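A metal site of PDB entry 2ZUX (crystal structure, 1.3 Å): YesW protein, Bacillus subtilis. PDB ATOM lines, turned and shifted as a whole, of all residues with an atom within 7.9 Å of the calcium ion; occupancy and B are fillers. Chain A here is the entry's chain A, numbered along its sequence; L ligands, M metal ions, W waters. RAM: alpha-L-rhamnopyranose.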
ATOM      1  N   ASN A 115      25.484  23.509  18.772  1.00  0.00           N
ATOM      2  CA  ASN A 115      24.720  23.828  19.969  1.00  0.00           C
ATOM      3  C   ASN A 115      24.267  22.513  20.629  1.00  0.00           C
ATOM      4  O   ASN A 115      25.065  21.571  20.715  1.00  0.00           O
ATOM      5  CB  ASN A 115      23.592  24.801  19.594  1.00  0.00           C
ATOM      6  CG  ASN A 115      23.014  25.547  20.788  1.00  0.00           C
ATOM      7  OD1 ASN A 115      23.557  26.589  21.227  1.00  0.00           O
ATOM      8  ND2 ASN A 115      21.894  25.073  21.275  1.00  0.00           N
ATOM      9  N   ASP A 116      23.016  22.441  21.094  1.00  0.00           N
ATOM     10  CA  ASP A 116      22.509  21.271  21.826  1.00  0.00           C
ATOM     11  C   ASP A 116      22.517  20.025  20.958  1.00  0.00           C
ATOM     12  O   ASP A 116      22.188  20.089  19.773  1.00  0.00           O
ATOM     13  CB  ASP A 116      21.071  21.510  22.275  1.00  0.00           C
ATOM     14  CG  ASP A 116      20.909  22.695  23.190  1.00  0.00           C
ATOM     15  OD1 ASP A 116      21.839  23.037  23.952  1.00  0.00           O
ATOM     16  OD2 ASP A 116      19.789  23.263  23.168  1.00  0.00           O
ATOM     17  N   ALA A 117      22.809  18.891  21.576  1.00  0.00           N
ATOM     18  CA  ALA A 117      22.694  17.608  20.910  1.00  0.00           C
ATOM     19  C   ALA A 117      21.802  16.641  21.671  1.00  0.00           C
ATOM     20  O   ALA A 117      21.441  16.852  22.837  1.00  0.00           O
ATOM     21  CB  ALA A 117      24.075  16.987  20.649  1.00  0.00           C
ATOM     22  N   LYS A 133      22.007  20.184  16.920  1.00  0.00           N
ATOM     23  CA  LYS A 133      21.340  21.416  16.516  1.00  0.00           C
ATOM     24  C   LYS A 133      22.402  22.493  16.324  1.00  0.00           C
ATOM     25  O   LYS A 133      23.240  22.714  17.193  1.00  0.00           O
ATOM     26  CB  LYS A 133      20.316  21.848  17.569  1.00  0.00           C
ATOM     27  CG  LYS A 133      19.542  23.127  17.218  1.00  0.00           C
ATOM     28  CD  LYS A 133      18.546  23.515  18.326  1.00  0.00           C
ATOM     29  CE  LYS A 133      19.288  24.094  19.518  1.00  0.00           C
ATOM     30  NZ  LYS A 133      18.380  24.364  20.687  1.00  0.00           N
ATOM     31  N   GLY A 175      16.102  29.922  18.547  1.00  0.00           N
ATOM     32  CA  GLY A 175      16.250  30.364  19.931  1.00  0.00           C
ATOM     33  C   GLY A 175      15.987  29.194  20.859  1.00  0.00           C
ATOM     34  O   GLY A 175      15.415  28.184  20.445  1.00  0.00           O
ATOM     35  N   ALA A 176      16.390  29.335  22.113  1.00  0.00           N
ATOM     36  CA  ALA A 176      16.338  28.223  23.075  1.00  0.00           C
ATOM     37  C   ALA A 176      14.945  27.621  23.236  1.00  0.00           C
ATOM     38  O   ALA A 176      14.817  26.414  23.475  1.00  0.00           O
ATOM     39  CB  ALA A 176      16.879  28.680  24.414  1.00  0.00           C
ATOM     40  N   HIS A 177      13.913  28.457  23.139  1.00  0.00           N
ATOM     41  CA  HIS A 177      12.572  28.047  23.519  1.00  0.00           C
ATOM     42  C   HIS A 177      11.717  27.598  22.361  1.00  0.00           C
ATOM     43  O   HIS A 177      10.566  27.220  22.565  1.00  0.00           O
ATOM     44  CB  HIS A 177      11.917  29.162  24.323  1.00  0.00           C
ATOM     45  CG  HIS A 177      12.724  29.548  25.508  1.00  0.00           C
ATOM     46  ND1 HIS A 177      12.899  28.709  26.588  1.00  0.00           N
ATOM     47  CD2 HIS A 177      13.520  30.619  25.726  1.00  0.00           C
ATOM     48  CE1 HIS A 177      13.716  29.275  27.452  1.00  0.00           C
ATOM     49  NE2 HIS A 177      14.107  30.437  26.945  1.00  0.00           N
ATOM     50  N   THR A 179      12.625  25.299  18.826  1.00  0.00           N
ATOM     51  CA  THR A 179      12.756  23.877  18.480  1.00  0.00           C
ATOM     52  C   THR A 179      13.213  23.055  19.674  1.00  0.00           C
ATOM     53  O   THR A 179      14.237  23.349  20.291  1.00  0.00           O
ATOM     54  CB  THR A 179      13.749  23.680  17.319  1.00  0.00           C
ATOM     55  OG1 THR A 179      13.262  24.368  16.170  1.00  0.00           O
ATOM     56  CG2 THR A 179      13.905  22.209  16.977  1.00  0.00           C
ATOM     57  N   GLN A 180      12.424  22.025  19.971  1.00  0.00           N
ATOM     58  CA  GLN A 180      12.692  21.032  21.011  1.00  0.00           C
ATOM     59  C   GLN A 180      12.653  19.672  20.326  1.00  0.00           C
ATOM     60  O   GLN A 180      11.594  19.234  19.893  1.00  0.00           O
ATOM     61  CB  GLN A 180      11.633  21.124  22.119  1.00  0.00           C
ATOM     62  CG  GLN A 180      11.333  22.553  22.603  1.00  0.00           C
ATOM     63  CD  GLN A 180      12.570  23.322  23.054  1.00  0.00           C
ATOM     64  OE1 GLN A 180      13.572  22.760  23.494  1.00  0.00           O
ATOM     65  NE2 GLN A 180      12.493  24.643  22.944  1.00  0.00           N
ATOM     66  N   PHE A 181      13.813  19.032  20.177  1.00  0.00           N
ATOM     67  CA  PHE A 181      13.888  17.845  19.327  1.00  0.00           C
ATOM     68  C   PHE A 181      14.055  16.557  20.107  1.00  0.00           C
ATOM     69  O   PHE A 181      14.918  16.435  20.970  1.00  0.00           O
ATOM     70  CB  PHE A 181      14.944  18.008  18.217  1.00  0.00           C
ATOM     71  CG  PHE A 181      16.370  18.207  18.709  1.00  0.00           C
ATOM     72  CD1 PHE A 181      17.277  17.170  18.649  1.00  0.00           C
ATOM     73  CD2 PHE A 181      16.800  19.454  19.176  1.00  0.00           C
ATOM     74  CE1 PHE A 181      18.599  17.341  19.084  1.00  0.00           C
ATOM     75  CE2 PHE A 181      18.112  19.621  19.627  1.00  0.00           C
ATOM     76  CZ  PHE A 181      19.002  18.569  19.577  1.00  0.00           C
ATOM     77  N   HIS A 326      11.376  26.366  32.345  1.00  0.00           N
ATOM     78  CA  HIS A 326      12.057  26.203  31.039  1.00  0.00           C
ATOM     79  C   HIS A 326      12.661  24.793  30.899  1.00  0.00           C
ATOM     80  O   HIS A 326      13.722  24.632  30.288  1.00  0.00           O
ATOM     81  CB  HIS A 326      13.207  27.189  30.867  1.00  0.00           C
ATOM     82  CG  HIS A 326      12.869  28.614  31.184  1.00  0.00           C
ATOM     83  ND1 HIS A 326      12.072  29.403  30.372  1.00  0.00           N
ATOM     84  CD2 HIS A 326      13.246  29.385  32.223  1.00  0.00           C
ATOM     85  CE1 HIS A 326      11.988  30.612  30.911  1.00  0.00           C
ATOM     86  NE2 HIS A 326      12.699  30.626  32.024  1.00  0.00           N
ATOM     87  N   ASN A 495      25.244  28.365  24.759  1.00  0.00           N
ATOM     88  CA  ASN A 495      24.076  29.025  25.337  1.00  0.00           C
ATOM     89  C   ASN A 495      24.402  30.132  26.327  1.00  0.00           C
ATOM     90  O   ASN A 495      23.727  30.296  27.339  1.00  0.00           O
ATOM     91  CB  ASN A 495      23.070  27.996  25.907  1.00  0.00           C
ATOM     92  CG  ASN A 495      22.597  27.009  24.856  1.00  0.00           C
ATOM     93  OD1 ASN A 495      22.549  25.782  25.102  1.00  0.00           O
ATOM     94  ND2 ASN A 495      22.245  27.515  23.699  1.00  0.00           N
ATOM     95  N   LYS A 498      24.213  30.250  30.245  1.00  0.00           N
ATOM     96  CA  LYS A 498      23.850  28.892  30.652  1.00  0.00           C
ATOM     97  C   LYS A 498      25.055  27.948  30.614  1.00  0.00           C
ATOM     98  O   LYS A 498      25.126  27.009  31.416  1.00  0.00           O
ATOM     99  CB  LYS A 498      22.702  28.345  29.806  1.00  0.00           C
ATOM    100  CG  LYS A 498      21.422  29.168  29.901  1.00  0.00           C
ATOM    101  CD  LYS A 498      20.799  29.143  31.305  1.00  0.00           C
ATOM    102  CE  LYS A 498      19.614  30.074  31.388  1.00  0.00           C
ATOM    103  NZ  LYS A 498      19.023  30.068  32.757  1.00  0.00           N
ATOM    104  N   THR A 500      26.327  25.442  28.812  1.00  0.00           N
ATOM    105  CA  THR A 500      26.001  24.017  28.785  1.00  0.00           C
ATOM    106  C   THR A 500      26.858  23.259  27.770  1.00  0.00           C
ATOM    107  O   THR A 500      27.219  23.806  26.732  1.00  0.00           O
ATOM    108  CB  THR A 500      24.509  23.798  28.439  1.00  0.00           C
ATOM    109  OG1 THR A 500      24.190  24.472  27.210  1.00  0.00           O
ATOM    110  CG2 THR A 500      23.623  24.333  29.564  1.00  0.00           C
ATOM    111  N   TRP A 553      15.479  14.596  26.926  1.00  0.00           N
ATOM    112  CA  TRP A 553      15.066  15.997  27.120  1.00  0.00           C
ATOM    113  C   TRP A 553      16.207  16.950  27.460  1.00  0.00           C
ATOM    114  O   TRP A 553      15.954  18.139  27.666  1.00  0.00           O
ATOM    115  CB  TRP A 553      13.877  16.171  28.086  1.00  0.00           C
ATOM    116  CG  TRP A 553      13.982  15.584  29.479  1.00  0.00           C
ATOM    117  CD1 TRP A 553      13.165  14.612  29.987  1.00  0.00           C
ATOM    118  CD2 TRP A 553      14.868  15.967  30.557  1.00  0.00           C
ATOM    119  NE1 TRP A 553      13.491  14.357  31.293  1.00  0.00           N
ATOM    120  CE2 TRP A 553      14.544  15.141  31.659  1.00  0.00           C
ATOM    121  CE3 TRP A 553      15.931  16.877  30.685  1.00  0.00           C
ATOM    122  CZ2 TRP A 553      15.230  15.228  32.881  1.00  0.00           C
ATOM    123  CZ3 TRP A 553      16.611  16.944  31.899  1.00  0.00           C
ATOM    124  CH2 TRP A 553      16.259  16.117  32.972  1.00  0.00           C
ATOM    125  N   GLN A 554      17.450  16.473  27.483  1.00  0.00           N
ATOM    126  CA  GLN A 554      18.543  17.369  27.888  1.00  0.00           C
ATOM    127  C   GLN A 554      18.587  18.646  27.055  1.00  0.00           C
ATOM    128  O   GLN A 554      18.818  19.740  27.591  1.00  0.00           O
ATOM    129  CB  GLN A 554      19.903  16.672  27.859  1.00  0.00           C
ATOM    130  CG  GLN A 554      20.981  17.517  28.540  1.00  0.00           C
ATOM    131  CD  GLN A 554      22.277  16.763  28.697  1.00  0.00           C
ATOM    132  OE1 GLN A 554      23.319  17.169  28.171  1.00  0.00           O
ATOM    133  NE2 GLN A 554      22.228  15.636  29.408  1.00  0.00           N
ATOM    134  N   ASN A 555      18.352  18.537  25.755  1.00  0.00           N
ATOM    135  CA  ASN A 555      18.431  19.710  24.895  1.00  0.00           C
ATOM    136  C   ASN A 555      17.373  20.766  25.178  1.00  0.00           C
ATOM    137  O   ASN A 555      17.570  21.924  24.851  1.00  0.00           O
ATOM    138  CB  ASN A 555      18.385  19.331  23.396  1.00  0.00           C
ATOM    139  CG  ASN A 555      17.015  18.815  22.960  1.00  0.00           C
ATOM    140  OD1 ASN A 555      16.757  17.599  22.974  1.00  0.00           O
ATOM    141  ND2 ASN A 555      16.174  19.712  22.492  1.00  0.00           N
ATOM    142  N   ILE A 556      16.234  20.352  25.727  1.00  0.00           N
ATOM    143  CA  ILE A 556      15.097  21.258  25.678  1.00  0.00           C
ATOM    144  C   ILE A 556      15.309  22.524  26.493  1.00  0.00           C
ATOM    145  O   ILE A 556      15.838  22.499  27.618  1.00  0.00           O
ATOM    146  CB  ILE A 556      13.757  20.578  26.008  1.00  0.00           C
ATOM    147  CG1 ILE A 556      13.586  20.374  27.502  1.00  0.00           C
ATOM    148  CG2 ILE A 556      13.594  19.289  25.193  1.00  0.00           C
ATOM    149  CD1 ILE A 556      12.219  19.827  27.882  1.00  0.00           C
ATOM    150  N   ALA A 557      14.918  23.624  25.868  1.00  0.00           N
ATOM    151  CA  ALA A 557      14.946  24.952  26.479  1.00  0.00           C
ATOM    152  C   ALA A 557      16.205  25.116  27.339  1.00  0.00           C
ATOM    153  O   ALA A 557      17.322  25.024  26.803  1.00  0.00           O
ATOM    154  CB  ALA A 557      13.649  25.229  27.248  1.00  0.00           C
ATOM    155  N   TYR A 558      16.079  25.375  28.634  1.00  0.00           N
ATOM    156  CA  TYR A 558      17.268  25.500  29.478  1.00  0.00           C
ATOM    157  C   TYR A 558      17.727  24.149  30.003  1.00  0.00           C
ATOM    158  O   TYR A 558      17.263  23.669  31.029  1.00  0.00           O
ATOM    159  CB  TYR A 558      17.054  26.514  30.609  1.00  0.00           C
ATOM    160  CG  TYR A 558      16.851  27.948  30.139  1.00  0.00           C
ATOM    161  CD1 TYR A 558      17.192  28.355  28.843  1.00  0.00           C
ATOM    162  CD2 TYR A 558      16.318  28.902  30.991  1.00  0.00           C
ATOM    163  CE1 TYR A 558      17.014  29.691  28.437  1.00  0.00           C
ATOM    164  CE2 TYR A 558      16.128  30.226  30.587  1.00  0.00           C
ATOM    165  CZ  TYR A 558      16.477  30.602  29.301  1.00  0.00           C
ATOM    166  OH  TYR A 558      16.305  31.894  28.853  1.00  0.00           O
ATOM    167  N   ASN A 559      18.668  23.580  29.249  1.00  0.00           N
ATOM    168  CA  ASN A 559      19.177  22.218  29.468  1.00  0.00           C
ATOM    169  C   ASN A 559      19.445  21.962  30.942  1.00  0.00           C
ATOM    170  O   ASN A 559      20.150  22.745  31.585  1.00  0.00           O
ATOM    171  CB  ASN A 559      20.526  22.012  28.759  1.00  0.00           C
ATOM    172  CG  ASN A 559      20.521  22.391  27.283  1.00  0.00           C
ATOM    173  OD1 ASN A 559      19.809  23.295  26.835  1.00  0.00           O
ATOM    174  ND2 ASN A 559      21.409  21.754  26.528  1.00  0.00           N
ATOM    175  N   GLN A 560      18.913  20.840  31.444  1.00  0.00           N
ATOM    176  CA  GLN A 560      19.145  20.386  32.826  1.00  0.00           C
ATOM    177  C   GLN A 560      19.882  19.051  32.807  1.00  0.00           C
ATOM    178  O   GLN A 560      19.740  18.296  31.843  1.00  0.00           O
ATOM    179  CB  GLN A 560      17.819  20.215  33.556  1.00  0.00           C
ATOM    180  CG  GLN A 560      17.042  21.513  33.721  1.00  0.00           C
ATOM    181  CD  GLN A 560      17.777  22.530  34.556  1.00  0.00           C
ATOM    182  OE1 GLN A 560      18.031  22.321  35.746  1.00  0.00           O
ATOM    183  NE2 GLN A 560      18.120  23.659  33.941  1.00  0.00           N
HETATM  184  C1  RAM L   1      19.940  31.729  26.034  1.00  0.00           C
HETATM  185  C2  RAM L   1      19.830  32.034  27.528  1.00  0.00           C
HETATM  186  C3  RAM L   1      21.170  32.507  28.091  1.00  0.00           C
HETATM  187  C4  RAM L   1      21.741  33.668  27.276  1.00  0.00           C
HETATM  188  C5  RAM L   1      21.789  33.279  25.797  1.00  0.00           C
HETATM  189  C6  RAM L   1      22.224  34.464  24.952  1.00  0.00           C
HETATM  190  O1  RAM L   1      20.674  30.541  25.833  1.00  0.00           O
HETATM  191  O2  RAM L   1      18.842  33.026  27.684  1.00  0.00           O
HETATM  192  O3  RAM L   1      21.035  32.890  29.445  1.00  0.00           O
HETATM  193  O4  RAM L   1      23.013  34.027  27.772  1.00  0.00           O
HETATM  194  O5  RAM L   1      20.529  32.815  25.331  1.00  0.00           O
HETATM  195 CA    CA M   1      18.478  24.026  24.971  1.00  0.00          CA
HETATM  196  O   HOH W   1      16.841  24.500  23.303  1.00  0.00           O
HETATM  197  O   HOH W   2      19.253  26.175  24.615  1.00  0.00           O
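The backbone carbonyl oxygen of Asn 495 sits at hydrogen-bond distance from an oxygen (O1) of the ligand, at 3.4 Å.
An oxygen (O2) of the ligand is in hydrogen-bond range of the side-chain hydroxyl of Tyr 558 (3.0 Å).
ND2 of Asn 559 lies close to O of Gln 554 (3.4 Å).
The side-chain amide oxygen of Asn 555 sits close to the backbone carbonyl oxygen of Phe 181.
The side-chain carboxylate (OD1) of Asp 116 lies close to the side-chain amide oxygen (OD1) of Asn 495, 3.1 Å away.
The backbone NH (N) of Lys 133 lies within hydrogen-bond range of the backbone carbonyl oxygen (O) of Asp 116.
The side-chain carboxylate (OD1) of Asp 116 sits close to the side-chain amide nitrogen (ND2) of Asn 115.
The backbone NH (N) of Ala 557 lies within hydrogen-bond range of the side-chain amide oxygen (OE1) of Gln 180 (2.9 Å).
Ile 556 touches the calcium ion (C to CA, 3.8 Å).
The nearest printed residue that does not touch the calcium ion is Lys 133 (4.3 Å).
The calcium ion is bound by the backbone carbonyl oxygen of Asn 555, water W2, the side-chain carboxylate of Asp 116, water W1, the backbone carbonyl oxygen of Ala 557 and the side-chain amide oxygen of Asn 559.
Water W1 lies within hydrogen-bond range of the backbone carbonyl oxygen (O) of Ala 176 (2.8 Å), the side-chain amino group (NZ) of Lys 133 (3.0 Å) and the backbone NH (N) of Ala 557 (3.3 Å).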
